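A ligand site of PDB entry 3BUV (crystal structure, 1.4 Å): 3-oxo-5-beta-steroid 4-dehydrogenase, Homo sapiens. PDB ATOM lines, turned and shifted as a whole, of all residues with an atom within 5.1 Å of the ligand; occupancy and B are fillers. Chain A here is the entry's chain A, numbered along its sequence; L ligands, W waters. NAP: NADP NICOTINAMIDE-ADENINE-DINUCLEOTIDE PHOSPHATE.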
ATOM      1  N   GLY A  24       0.294 -23.419  29.536  1.00  0.00           N
ATOM      2  CA  GLY A  24      -0.498 -24.367  28.786  1.00  0.00           C
ATOM      3  C   GLY A  24      -0.183 -24.145  27.318  1.00  0.00           C
ATOM      4  O   GLY A  24       0.148 -23.029  26.917  1.00  0.00           O
ATOM      5  N   THR A  25      -0.285 -25.189  26.498  1.00  0.00           N
ATOM      6  CA  THR A  25       0.048 -25.048  25.095  1.00  0.00           C
ATOM      7  C   THR A  25      -1.009 -25.497  24.092  1.00  0.00           C
ATOM      8  O   THR A  25      -0.701 -25.673  22.909  1.00  0.00           O
ATOM      9  CB  THR A  25       1.377 -25.757  24.771  1.00  0.00           C
ATOM     10  OG1 THR A  25       1.273 -27.148  25.084  1.00  0.00           O
ATOM     11  CG2 THR A  25       2.527 -25.134  25.558  1.00  0.00           C
ATOM     12  N   TYR A  26      -2.239 -25.699  24.545  1.00  0.00           N
ATOM     13  CA  TYR A  26      -3.267 -26.072  23.598  1.00  0.00           C
ATOM     14  C   TYR A  26      -3.644 -24.827  22.806  1.00  0.00           C
ATOM     15  O   TYR A  26      -3.835 -23.741  23.374  1.00  0.00           O
ATOM     16  CB  TYR A  26      -4.523 -26.608  24.299  1.00  0.00           C
ATOM     17  CG  TYR A  26      -5.732 -26.631  23.394  1.00  0.00           C
ATOM     18  CD1 TYR A  26      -5.724 -27.364  22.194  1.00  0.00           C
ATOM     19  CD2 TYR A  26      -6.881 -25.897  23.697  1.00  0.00           C
ATOM     20  CE1 TYR A  26      -6.821 -27.357  21.335  1.00  0.00           C
ATOM     21  CE2 TYR A  26      -7.990 -25.890  22.845  1.00  0.00           C
ATOM     22  CZ  TYR A  26      -7.938 -26.617  21.668  1.00  0.00           C
ATOM     23  OH  TYR A  26      -9.027 -26.604  20.810  1.00  0.00           O
ATOM     24  N   ASP A  53       2.895 -27.425  29.971  1.00  0.00           N
ATOM     25  CA  ASP A  53       1.902 -28.487  29.843  1.00  0.00           C
ATOM     26  C   ASP A  53       1.564 -28.625  28.372  1.00  0.00           C
ATOM     27  O   ASP A  53       1.204 -27.650  27.716  1.00  0.00           O
ATOM     28  CB  ASP A  53       0.629 -28.151  30.617  1.00  0.00           C
ATOM     29  CG  ASP A  53      -0.420 -29.237  30.487  1.00  0.00           C
ATOM     30  OD1 ASP A  53      -0.337 -30.225  31.223  1.00  0.00           O
ATOM     31  OD2 ASP A  53      -1.306 -29.094  29.622  1.00  0.00           O
ATOM     32  N   GLY A  54       1.672 -29.856  27.858  1.00  0.00           N
ATOM     33  CA  GLY A  54       1.372 -30.085  26.459  1.00  0.00           C
ATOM     34  C   GLY A  54       0.781 -31.438  26.193  1.00  0.00           C
ATOM     35  O   GLY A  54       0.449 -32.188  27.117  1.00  0.00           O
ATOM     36  N   TYR A  58      -2.004 -31.986  20.491  1.00  0.00           N
ATOM     37  CA  TYR A  58      -2.143 -30.539  20.295  1.00  0.00           C
ATOM     38  C   TYR A  58      -1.411 -30.168  19.000  1.00  0.00           C
ATOM     39  O   TYR A  58      -1.479 -29.027  18.539  1.00  0.00           O
ATOM     40  CB  TYR A  58      -1.537 -29.748  21.463  1.00  0.00           C
ATOM     41  CG  TYR A  58      -2.244 -29.899  22.807  1.00  0.00           C
ATOM     42  CD1 TYR A  58      -3.443 -30.604  22.931  1.00  0.00           C
ATOM     43  CD2 TYR A  58      -1.688 -29.345  23.953  1.00  0.00           C
ATOM     44  CE1 TYR A  58      -4.060 -30.772  24.173  1.00  0.00           C
ATOM     45  CE2 TYR A  58      -2.294 -29.496  25.203  1.00  0.00           C
ATOM     46  CZ  TYR A  58      -3.471 -30.212  25.306  1.00  0.00           C
ATOM     47  OH  TYR A  58      -4.039 -30.397  26.550  1.00  0.00           O
ATOM     48  N   LYS A  87       0.554 -36.128  27.605  1.00  0.00           N
ATOM     49  CA  LYS A  87      -0.678 -36.862  27.848  1.00  0.00           C
ATOM     50  C   LYS A  87      -0.965 -38.001  26.872  1.00  0.00           C
ATOM     51  O   LYS A  87      -0.635 -37.917  25.689  1.00  0.00           O
ATOM     52  CB  LYS A  87      -1.857 -35.882  27.824  1.00  0.00           C
ATOM     53  CG  LYS A  87      -1.579 -34.582  28.573  1.00  0.00           C
ATOM     54  CD  LYS A  87      -2.847 -33.780  28.786  1.00  0.00           C
ATOM     55  CE  LYS A  87      -2.557 -32.458  29.451  1.00  0.00           C
ATOM     56  NZ  LYS A  87      -1.978 -31.469  28.501  1.00  0.00           N
ATOM     57  N   GLU A 120      -4.956 -38.748  29.436  1.00  0.00           N
ATOM     58  CA  GLU A 120      -5.664 -37.528  29.034  1.00  0.00           C
ATOM     59  C   GLU A 120      -7.143 -37.467  29.412  1.00  0.00           C
ATOM     60  O   GLU A 120      -7.630 -36.425  29.855  1.00  0.00           O
ATOM     61  CB  GLU A 120      -5.482 -37.325  27.526  1.00  0.00           C
ATOM     62  CG  GLU A 120      -5.699 -35.892  27.058  1.00  0.00           C
ATOM     63  CD  GLU A 120      -4.828 -35.530  25.861  1.00  0.00           C
ATOM     64  OE1 GLU A 120      -4.285 -36.451  25.208  1.00  0.00           O
ATOM     65  OE2 GLU A 120      -4.699 -34.329  25.564  1.00  0.00           O
ATOM     66  N   VAL A 121      -7.862 -38.561  29.210  1.00  0.00           N
ATOM     67  CA  VAL A 121      -9.273 -38.661  29.577  1.00  0.00           C
ATOM     68  C   VAL A 121      -9.458 -40.116  29.980  1.00  0.00           C
ATOM     69  O   VAL A 121      -8.734 -40.988  29.518  1.00  0.00           O
ATOM     70  CB  VAL A 121     -10.226 -38.342  28.405  1.00  0.00           C
ATOM     71  CG1 VAL A 121     -10.202 -36.842  28.109  1.00  0.00           C
ATOM     72  CG2 VAL A 121      -9.844 -39.129  27.171  1.00  0.00           C
ATOM     73  N   SER A 169      -6.112 -37.260  34.124  1.00  0.00           N
ATOM     74  CA  SER A 169      -6.814 -36.034  33.779  1.00  0.00           C
ATOM     75  C   SER A 169      -8.283 -36.346  33.515  1.00  0.00           C
ATOM     76  O   SER A 169      -8.601 -37.339  32.876  1.00  0.00           O
ATOM     77  CB  SER A 169      -6.182 -35.392  32.542  1.00  0.00           C
ATOM     78  OG  SER A 169      -6.819 -34.171  32.214  1.00  0.00           O
ATOM     79  N   ASN A 170      -9.155 -35.475  34.013  1.00  0.00           N
ATOM     80  CA  ASN A 170     -10.596 -35.642  33.834  1.00  0.00           C
ATOM     81  C   ASN A 170     -11.124 -36.909  34.498  1.00  0.00           C
ATOM     82  O   ASN A 170     -12.062 -37.533  34.009  1.00  0.00           O
ATOM     83  CB  ASN A 170     -10.943 -35.647  32.334  1.00  0.00           C
ATOM     84  CG  ASN A 170     -10.678 -34.307  31.674  1.00  0.00           C
ATOM     85  OD1 ASN A 170     -11.299 -33.296  32.012  1.00  0.00           O
ATOM     86  ND2 ASN A 170      -9.760 -34.296  30.714  1.00  0.00           N
ATOM     87  N   GLN A 193      -5.462 -33.645  36.548  1.00  0.00           N
ATOM     88  CA  GLN A 193      -5.639 -32.374  35.835  1.00  0.00           C
ATOM     89  C   GLN A 193      -7.086 -32.230  35.407  1.00  0.00           C
ATOM     90  O   GLN A 193      -7.578 -32.973  34.562  1.00  0.00           O
ATOM     91  CB  GLN A 193      -4.719 -32.318  34.620  1.00  0.00           C
ATOM     92  CG  GLN A 193      -4.694 -30.952  33.943  1.00  0.00           C
ATOM     93  CD  GLN A 193      -3.779 -30.891  32.734  1.00  0.00           C
ATOM     94  OE1 GLN A 193      -4.234 -30.681  31.611  1.00  0.00           O
ATOM     95  NE2 GLN A 193      -2.483 -31.072  32.965  1.00  0.00           N
ATOM     96  N   TYR A 219      -6.721 -26.998  34.678  1.00  0.00           N
ATOM     97  CA  TYR A 219      -6.675 -26.664  33.263  1.00  0.00           C
ATOM     98  C   TYR A 219      -7.727 -25.625  33.039  1.00  0.00           C
ATOM     99  O   TYR A 219      -8.668 -25.511  33.835  1.00  0.00           O
ATOM    100  CB  TYR A 219      -6.776 -27.911  32.380  1.00  0.00           C
ATOM    101  CG  TYR A 219      -8.108 -28.619  32.158  1.00  0.00           C
ATOM    102  CD1 TYR A 219      -9.215 -27.981  31.579  1.00  0.00           C
ATOM    103  CD2 TYR A 219      -8.232 -29.964  32.463  1.00  0.00           C
ATOM    104  CE1 TYR A 219     -10.393 -28.677  31.286  1.00  0.00           C
ATOM    105  CE2 TYR A 219      -9.389 -30.688  32.164  1.00  0.00           C
ATOM    106  CZ  TYR A 219     -10.455 -30.038  31.573  1.00  0.00           C
ATOM    107  OH  TYR A 219     -11.594 -30.734  31.246  1.00  0.00           O
ATOM    108  N   SER A 220      -7.611 -24.844  31.978  1.00  0.00           N
ATOM    109  CA  SER A 220      -8.547 -23.758  31.702  1.00  0.00           C
ATOM    110  C   SER A 220      -8.686 -22.917  32.974  1.00  0.00           C
ATOM    111  O   SER A 220      -9.805 -22.552  33.358  1.00  0.00           O
ATOM    112  CB  SER A 220      -9.909 -24.312  31.273  1.00  0.00           C
ATOM    113  OG  SER A 220      -9.791 -25.061  30.085  1.00  0.00           O
ATOM    114  N   PRO A 221      -7.556 -22.584  33.627  1.00  0.00           N
ATOM    115  CA  PRO A 221      -7.607 -21.793  34.867  1.00  0.00           C
ATOM    116  C   PRO A 221      -8.113 -20.368  34.670  1.00  0.00           C
ATOM    117  O   PRO A 221      -8.439 -19.679  35.645  1.00  0.00           O
ATOM    118  CB  PRO A 221      -6.172 -21.856  35.365  1.00  0.00           C
ATOM    119  CG  PRO A 221      -5.393 -21.825  34.080  1.00  0.00           C
ATOM    120  CD  PRO A 221      -6.163 -22.796  33.204  1.00  0.00           C
ATOM    121  N   LEU A 222      -8.165 -19.924  33.421  1.00  0.00           N
ATOM    122  CA  LEU A 222      -8.645 -18.579  33.105  1.00  0.00           C
ATOM    123  C   LEU A 222     -10.042 -18.632  32.496  1.00  0.00           C
ATOM    124  O   LEU A 222     -10.551 -17.629  31.997  1.00  0.00           O
ATOM    125  CB  LEU A 222      -7.686 -17.875  32.144  1.00  0.00           C
ATOM    126  CG  LEU A 222      -6.276 -17.632  32.674  1.00  0.00           C
ATOM    127  CD1 LEU A 222      -5.473 -16.895  31.614  1.00  0.00           C
ATOM    128  CD2 LEU A 222      -6.322 -16.835  33.971  1.00  0.00           C
ATOM    129  N   GLY A 223     -10.659 -19.811  32.533  1.00  0.00           N
ATOM    130  CA  GLY A 223     -11.993 -19.954  31.997  1.00  0.00           C
ATOM    131  C   GLY A 223     -12.108 -20.349  30.537  1.00  0.00           C
ATOM    132  O   GLY A 223     -13.185 -20.231  29.961  1.00  0.00           O
ATOM    133  N   THR A 224     -11.009 -20.831  29.961  1.00  0.00           N
ATOM    134  CA  THR A 224     -10.926 -21.281  28.558  1.00  0.00           C
ATOM    135  C   THR A 224     -10.847 -20.160  27.523  1.00  0.00           C
ATOM    136  O   THR A 224     -11.069 -18.983  27.834  1.00  0.00           O
ATOM    137  CB  THR A 224     -12.128 -22.174  28.123  1.00  0.00           C
ATOM    138  OG1 THR A 224     -13.251 -21.356  27.776  1.00  0.00           O
ATOM    139  CG2 THR A 224     -12.523 -23.137  29.243  1.00  0.00           C
ATOM    140  N   SER A 225     -10.543 -20.549  26.284  1.00  0.00           N
ATOM    141  CA  SER A 225     -10.467 -19.607  25.165  1.00  0.00           C
ATOM    142  C   SER A 225     -11.865 -19.370  24.619  1.00  0.00           C
ATOM    143  O   SER A 225     -12.057 -18.644  23.638  1.00  0.00           O
ATOM    144  CB  SER A 225      -9.573 -20.185  24.058  1.00  0.00           C
ATOM    145  OG  SER A 225     -10.119 -21.383  23.545  1.00  0.00           O
ATOM    146  N   LEU A 239     -13.374 -14.017  33.203  1.00  0.00           N
ATOM    147  CA  LEU A 239     -12.573 -12.812  33.380  1.00  0.00           C
ATOM    148  C   LEU A 239     -13.345 -11.509  33.420  1.00  0.00           C
ATOM    149  O   LEU A 239     -12.764 -10.446  33.617  1.00  0.00           O
ATOM    150  CB  LEU A 239     -11.480 -12.765  32.313  1.00  0.00           C
ATOM    151  CG  LEU A 239     -10.524 -13.967  32.336  1.00  0.00           C
ATOM    152  CD1 LEU A 239      -9.418 -13.752  31.326  1.00  0.00           C
ATOM    153  CD2 LEU A 239      -9.949 -14.150  33.733  1.00  0.00           C
ATOM    154  N   THR A 254      -4.983  -7.724  37.066  1.00  0.00           N
ATOM    155  CA  THR A 254      -6.096  -8.052  36.186  1.00  0.00           C
ATOM    156  C   THR A 254      -6.865  -9.206  36.818  1.00  0.00           C
ATOM    157  O   THR A 254      -6.359  -9.884  37.712  1.00  0.00           O
ATOM    158  CB  THR A 254      -5.617  -8.486  34.792  1.00  0.00           C
ATOM    159  OG1 THR A 254      -4.825  -9.672  34.915  1.00  0.00           O
ATOM    160  CG2 THR A 254      -4.786  -7.383  34.142  1.00  0.00           C
ATOM    161  N   ALA A 256      -7.420 -11.938  35.533  1.00  0.00           N
ATOM    162  CA  ALA A 256      -6.663 -13.155  35.237  1.00  0.00           C
ATOM    163  C   ALA A 256      -5.643 -13.428  36.341  1.00  0.00           C
ATOM    164  O   ALA A 256      -5.477 -14.550  36.792  1.00  0.00           O
ATOM    165  CB  ALA A 256      -5.964 -13.027  33.892  1.00  0.00           C
ATOM    166  N   ILE A 271      -2.148 -23.911  34.923  1.00  0.00           N
ATOM    167  CA  ILE A 271      -1.429 -23.949  33.657  1.00  0.00           C
ATOM    168  C   ILE A 271      -2.090 -23.067  32.593  1.00  0.00           C
ATOM    169  O   ILE A 271      -2.503 -23.532  31.524  1.00  0.00           O
ATOM    170  CB  ILE A 271      -1.298 -25.400  33.124  1.00  0.00           C
ATOM    171  CG1 ILE A 271      -2.655 -26.119  33.128  1.00  0.00           C
ATOM    172  CG2 ILE A 271      -0.303 -26.170  33.989  1.00  0.00           C
ATOM    173  CD1 ILE A 271      -2.628 -27.484  32.441  1.00  0.00           C
ATOM    174  N   PRO A 272      -2.181 -21.761  32.867  1.00  0.00           N
ATOM    175  CA  PRO A 272      -2.790 -20.837  31.918  1.00  0.00           C
ATOM    176  C   PRO A 272      -2.053 -20.812  30.582  1.00  0.00           C
ATOM    177  O   PRO A 272      -0.809 -20.822  30.548  1.00  0.00           O
ATOM    178  CB  PRO A 272      -2.716 -19.493  32.644  1.00  0.00           C
ATOM    179  CG  PRO A 272      -1.456 -19.638  33.461  1.00  0.00           C
ATOM    180  CD  PRO A 272      -1.590 -21.034  34.006  1.00  0.00           C
ATOM    181  N   LYS A 273      -2.815 -20.762  29.510  1.00  0.00           N
ATOM    182  CA  LYS A 273      -2.233 -20.710  28.168  1.00  0.00           C
ATOM    183  C   LYS A 273      -2.297 -19.328  27.565  1.00  0.00           C
ATOM    184  O   LYS A 273      -3.332 -18.652  27.612  1.00  0.00           O
ATOM    185  CB  LYS A 273      -2.957 -21.693  27.230  1.00  0.00           C
ATOM    186  CG  LYS A 273      -2.537 -21.597  25.746  1.00  0.00           C
ATOM    187  CD  LYS A 273      -3.266 -20.482  24.969  1.00  0.00           C
ATOM    188  CE  LYS A 273      -2.826 -20.433  23.507  1.00  0.00           C
ATOM    189  NZ  LYS A 273      -3.595 -19.400  22.742  1.00  0.00           N
ATOM    190  N   SER A 274      -1.184 -18.891  27.000  1.00  0.00           N
ATOM    191  CA  SER A 274      -1.132 -17.630  26.282  1.00  0.00           C
ATOM    192  C   SER A 274       0.020 -17.685  25.310  1.00  0.00           C
ATOM    193  O   SER A 274       1.114 -18.122  25.654  1.00  0.00           O
ATOM    194  CB  SER A 274      -0.913 -16.428  27.206  1.00  0.00           C
ATOM    195  OG  SER A 274      -0.820 -15.253  26.412  1.00  0.00           O
ATOM    196  N   PHE A 275      -0.237 -17.267  24.081  1.00  0.00           N
ATOM    197  CA  PHE A 275       0.793 -17.220  23.061  1.00  0.00           C
ATOM    198  C   PHE A 275       1.047 -15.746  22.747  1.00  0.00           C
ATOM    199  O   PHE A 275       1.573 -15.394  21.698  1.00  0.00           O
ATOM    200  CB  PHE A 275       0.379 -17.981  21.802  1.00  0.00           C
ATOM    201  CG  PHE A 275       0.514 -19.486  21.913  1.00  0.00           C
ATOM    202  CD1 PHE A 275       0.220 -20.303  20.822  1.00  0.00           C
ATOM    203  CD2 PHE A 275       0.955 -20.088  23.080  1.00  0.00           C
ATOM    204  CE1 PHE A 275       0.346 -21.693  20.904  1.00  0.00           C
ATOM    205  CE2 PHE A 275       1.092 -21.477  23.184  1.00  0.00           C
ATOM    206  CZ  PHE A 275       0.787 -22.277  22.085  1.00  0.00           C
ATOM    207  N   ASN A 276       0.656 -14.897  23.690  1.00  0.00           N
ATOM    208  CA  ASN A 276       0.838 -13.453  23.556  1.00  0.00           C
ATOM    209  C   ASN A 276       1.921 -13.021  24.533  1.00  0.00           C
ATOM    210  O   ASN A 276       1.839 -13.310  25.727  1.00  0.00           O
ATOM    211  CB  ASN A 276      -0.490 -12.744  23.853  1.00  0.00           C
ATOM    212  CG  ASN A 276      -0.349 -11.235  23.902  1.00  0.00           C
ATOM    213  OD1 ASN A 276       0.065 -10.666  24.914  1.00  0.00           O
ATOM    214  ND2 ASN A 276      -0.687 -10.574  22.795  1.00  0.00           N
ATOM    215  N   ARG A 279       0.668 -11.085  27.764  1.00  0.00           N
ATOM    216  CA  ARG A 279      -0.127 -11.909  28.655  1.00  0.00           C
ATOM    217  C   ARG A 279       0.656 -13.058  29.294  1.00  0.00           C
ATOM    218  O   ARG A 279       0.369 -13.454  30.416  1.00  0.00           O
ATOM    219  CB  ARG A 279      -1.387 -12.417  27.934  1.00  0.00           C
ATOM    220  CG  ARG A 279      -2.328 -11.268  27.558  1.00  0.00           C
ATOM    221  CD  ARG A 279      -3.675 -11.753  27.052  1.00  0.00           C
ATOM    222  NE  ARG A 279      -3.634 -12.232  25.675  1.00  0.00           N
ATOM    223  CZ  ARG A 279      -3.677 -11.453  24.602  1.00  0.00           C
ATOM    224  NH1 ARG A 279      -3.750 -10.130  24.742  1.00  0.00           N
ATOM    225  NH2 ARG A 279      -3.666 -11.984  23.380  1.00  0.00           N
ATOM    226  N   GLU A 282       2.193 -11.302  32.102  1.00  0.00           N
ATOM    227  CA  GLU A 282       1.149 -10.933  33.056  1.00  0.00           C
ATOM    228  C   GLU A 282       0.725 -12.100  33.949  1.00  0.00           C
ATOM    229  O   GLU A 282       0.646 -11.968  35.156  1.00  0.00           O
ATOM    230  CB  GLU A 282      -0.064 -10.378  32.303  1.00  0.00           C
ATOM    231  CG  GLU A 282      -1.311 -10.151  33.157  1.00  0.00           C
ATOM    232  CD  GLU A 282      -2.500  -9.712  32.328  1.00  0.00           C
ATOM    233  OE1 GLU A 282      -3.635 -10.138  32.623  1.00  0.00           O
ATOM    234  OE2 GLU A 282      -2.310  -8.917  31.377  1.00  0.00           O
ATOM    235  N   ASN A 283       0.468 -13.249  33.335  1.00  0.00           N
ATOM    236  CA  ASN A 283       0.041 -14.422  34.101  1.00  0.00           C
ATOM    237  C   ASN A 283       1.056 -14.920  35.114  1.00  0.00           C
ATOM    238  O   ASN A 283       0.697 -15.583  36.079  1.00  0.00           O
ATOM    239  CB  ASN A 283      -0.344 -15.562  33.149  1.00  0.00           C
ATOM    240  CG  ASN A 283      -1.496 -15.186  32.237  1.00  0.00           C
ATOM    241  OD1 ASN A 283      -2.270 -14.269  32.541  1.00  0.00           O
ATOM    242  ND2 ASN A 283      -1.652 -15.903  31.137  1.00  0.00           N
HETATM  243  PA  NAP L   1      -7.100 -20.894  29.711  1.00  0.00           P
HETATM  244  O1A NAP L   1      -8.077 -20.894  30.725  1.00  0.00           O
HETATM  245  O2A NAP L   1      -5.653 -21.033  30.032  1.00  0.00           O
HETATM  246  O5B NAP L   1      -7.377 -19.608  28.760  1.00  0.00           O
HETATM  247  C5B NAP L   1      -6.816 -19.371  27.656  1.00  0.00           C
HETATM  248  C4B NAP L   1      -7.435 -18.232  26.812  1.00  0.00           C
HETATM  249  O4B NAP L   1      -7.181 -17.088  27.575  1.00  0.00           O
HETATM  250  C3B NAP L   1      -6.725 -17.965  25.460  1.00  0.00           C
HETATM  251  O3B NAP L   1      -7.747 -17.548  24.553  1.00  0.00           O
HETATM  252  C2B NAP L   1      -5.724 -16.873  25.772  1.00  0.00           C
HETATM  253  O2B NAP L   1      -5.440 -16.062  24.606  1.00  0.00           O
HETATM  254  C1B NAP L   1      -6.416 -16.079  26.873  1.00  0.00           C
HETATM  255  N9A NAP L   1      -5.577 -15.465  27.888  1.00  0.00           N
HETATM  256  C8A NAP L   1      -4.388 -15.905  28.413  1.00  0.00           C
HETATM  257  N7A NAP L   1      -3.889 -15.041  29.364  1.00  0.00           N
HETATM  258  C5A NAP L   1      -4.832 -14.081  29.392  1.00  0.00           C
HETATM  259  C6A NAP L   1      -4.833 -12.911  30.201  1.00  0.00           C
HETATM  260  N6A NAP L   1      -3.947 -12.528  31.092  1.00  0.00           N
HETATM  261  N1A NAP L   1      -5.971 -12.029  30.009  1.00  0.00           N
HETATM  262  C2A NAP L   1      -6.998 -12.287  29.112  1.00  0.00           C
HETATM  263  N3A NAP L   1      -6.959 -13.410  28.347  1.00  0.00           N
HETATM  264  C4A NAP L   1      -5.843 -14.327  28.495  1.00  0.00           C
HETATM  265  O3  NAP L   1      -7.382 -22.200  28.877  1.00  0.00           O
HETATM  266  PN  NAP L   1      -6.993 -23.521  28.212  1.00  0.00           P
HETATM  267  O1N NAP L   1      -8.156 -24.217  27.856  1.00  0.00           O
HETATM  268  O2N NAP L   1      -6.005 -23.158  27.132  1.00  0.00           O
HETATM  269  O5D NAP L   1      -6.294 -24.068  29.354  1.00  0.00           O
HETATM  270  C5D NAP L   1      -4.940 -24.138  29.834  1.00  0.00           C
HETATM  271  C4D NAP L   1      -4.105 -25.303  29.399  1.00  0.00           C
HETATM  272  O4D NAP L   1      -4.710 -26.479  30.038  1.00  0.00           O
HETATM  273  C3D NAP L   1      -4.198 -25.727  27.890  1.00  0.00           C
HETATM  274  O3D NAP L   1      -3.599 -24.767  26.976  1.00  0.00           O
HETATM  275  C2D NAP L   1      -3.692 -27.165  28.009  1.00  0.00           C
HETATM  276  O2D NAP L   1      -2.243 -27.125  28.124  1.00  0.00           O
HETATM  277  C1D NAP L   1      -4.468 -27.658  29.232  1.00  0.00           C
HETATM  278  N1N NAP L   1      -5.842 -28.257  29.008  1.00  0.00           N
HETATM  279  C2N NAP L   1      -6.012 -29.626  29.333  1.00  0.00           C
HETATM  280  C3N NAP L   1      -7.282 -30.247  29.078  1.00  0.00           C
HETATM  281  C7N NAP L   1      -7.468 -31.731  29.431  1.00  0.00           C
HETATM  282  O7N NAP L   1      -8.540 -32.269  29.205  1.00  0.00           O
HETATM  283  N7N NAP L   1      -6.364 -32.260  29.959  1.00  0.00           N
HETATM  284  C4N NAP L   1      -8.374 -29.494  28.499  1.00  0.00           C
HETATM  285  C5N NAP L   1      -8.245 -28.068  28.173  1.00  0.00           C
HETATM  286  C6N NAP L   1      -6.996 -27.487  28.434  1.00  0.00           C
HETATM  287  P2B NAP L   1      -3.929 -15.655  24.206  1.00  0.00           P
HETATM  288  O1X NAP L   1      -3.100 -16.923  23.955  1.00  0.00           O
HETATM  289  O2X NAP L   1      -4.116 -14.820  22.949  1.00  0.00           O
HETATM  290  O3X NAP L   1      -3.340 -14.892  25.387  1.00  0.00           O
HETATM  291  O   HOH W   1      -5.721 -32.331  26.752  1.00  0.00           O
HETATM  292  O   HOH W   2      -9.669 -14.494  27.667  1.00  0.00           O
HETATM  293  O   HOH W   3      -6.026  -9.621  31.391  1.00  0.00           O
HETATM  294  O   HOH W   4      -6.747 -22.161  24.727  1.00  0.00           O
HETATM  295  O   HOH W   5      -5.156 -16.147  20.683  1.00  0.00           O
HETATM  296  O   HOH W   6      -9.965 -15.779  25.148  1.00  0.00           O
HETATM  297  O   HOH W   7      -8.551 -32.237  26.275  1.00  0.00           O
HETATM  298  O   HOH W   8      -9.769 -23.510  25.933  1.00  0.00           O
HETATM  299  O   HOH W   9      -6.887 -18.012  22.135  1.00  0.00           O
HETATM  300  O   HOH W  10      -2.008 -15.181  21.162  1.00  0.00           O
HETATM  301  O   HOH W  11      -6.767 -13.799  22.567  1.00  0.00           O
HETATM  302  O   HOH W  12     -11.149 -31.712  28.424  1.00  0.00           O
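O2D of the ligand is in hydrogen-bond range of OD2 of Asp 53 (2.6 Å). NE of Arg 279 is in salt-bridge range of O3X of the ligand. The side-chain hydroxyl of Ser 274 sits at hydrogen-bond distance from an oxygen (O3X) of the ligand (2.7 Å). An oxygen (O2A) of the ligand lies within hydrogen-bond range of the backbone NH (N) of Lys 273 (2.9 Å). NZ of Lys 273 lies within salt-bridge range of O1X of the ligand, 2.8 Å away. The side-chain amide nitrogen of Asn 170 is in hydrogen-bond range of an oxygen (O7N) of the ligand (2.8 Å). A nitrogen (N6A) of the ligand lies within hydrogen-bond range of the side-chain amide oxygen of Asn 283 (2.8 Å). N6A of the ligand is in hydrogen-bond range of OE1 of Glu 282 (2.9 Å). N of Leu 222 lies within hydrogen-bond range of O1A of the ligand. The backbone NH (N) of Phe 275 is in hydrogen-bond range of an oxygen (O1X) of the ligand, at 2.9 Å. N of Ser 220 lies within hydrogen-bond range of O5D of the ligand, at 3.0 Å. An oxygen (O1N) of the ligand lies within hydrogen-bond range of the side-chain hydroxyl (OG) of Ser 220, 2.9 Å away. The backbone NH (N) of Tyr 26 sits at hydrogen-bond distance from an oxygen (O3D) of the ligand (2.9 Å). The side-chain hydroxyl of Ser 169 sits at hydrogen-bond distance from a nitrogen (N7N) of the ligand. The backbone NH of Thr 224 sits at hydrogen-bond distance from an oxygen (O1A) of the ligand (3.0 Å). The side-chain amide oxygen (OE1) of Gln 193 sits close to a nitrogen (N7N) of the ligand. O2D of the ligand sits at hydrogen-bond distance from N of Thr 25 (3.2 Å). An oxygen (O1A) of the ligand lies within hydrogen-bond range of the backbone NH of Gly 223.
An oxygen (O1A) of the ligand lies close to the backbone nitrogen (N) of Pro 221. Residues that only touch the ligand: Ile 271 (3.0 Å), Ser 225 (3.2 Å), Gly 24 (3.3 Å), Pro 272 (3.4 Å), Tyr 219 (3.4 Å), Ala 256 (3.5 Å), Tyr 58 (3.5 Å), Leu 239 (3.6 Å), Lys 87 (3.8 Å) and Asn 276 (3.9 Å). Hydrophobic or aromatic side chains within 4 Å of the ligand: Tyr 26, Tyr 58, Tyr 219, Pro 221, Leu 222, Leu 239, Ala 256 and Ile 271. Within 4 Å of the ligand: Gly 24, Thr 25, Tyr 26, Asp 53, Tyr 58, Lys 87, Ser 169, Asn 170, Gln 193, Tyr 219, Ser 220, Pro 221, Leu 222, Gly 223, Thr 224, Ser 225, Leu 239, Ala 256, Ile 271, Pro 272, Lys 273, Ser 274, Phe 275, Asn 276, Arg 279, Glu 282 and Asn 283.
Water W8 lies within hydrogen-bond range of O1N of the ligand (2.6 Å) and N of Ser 225 (3.1 Å). Water W3 lies within hydrogen-bond range of OE1 of Glu 282 (2.7 Å) and N1A of the ligand (2.8 Å). Water W12 lies within hydrogen-bond range of an oxygen (O7N) of the ligand (2.8 Å) and the side-chain hydroxyl of Tyr 219 (3.0 Å). Water W1 lies within hydrogen-bond range of OE2 of Glu 120 (2.5 Å), OH of Tyr 58 (2.6 Å) and N7N of the ligand (3.3 Å).
The side-chain hydroxyl (OG1) of Thr 25 lies within hydrogen-bond range of the backbone carbonyl oxygen (O) of Asp 53, 2.7 Å away. The side-chain carboxylate (OD2) of Asp 53 is in salt-bridge range of the side-chain amino group (NZ) of Lys 87 (2.7 Å). The side-chain amide nitrogen of Asn 170 sits at hydrogen-bond distance from the backbone carbonyl oxygen of Glu 120 (3.1 Å). The side-chain hydroxyl of Thr 254 is in hydrogen-bond range of the side-chain carboxylate of Glu 282. O of Ile 271 is in hydrogen-bond range of N of Gly 24 (3.4 Å). N of Gly 24 lies within hydrogen-bond range of O of Pro 272 (3.0 Å). The backbone NH of Ala 256 lies close to the side-chain hydroxyl of Thr 254 (3.5 Å). The side-chain hydroxyl (OH) of Tyr 58 sits at hydrogen-bond distance from the side-chain amino group (NZ) of Lys 87 (3.0 Å).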
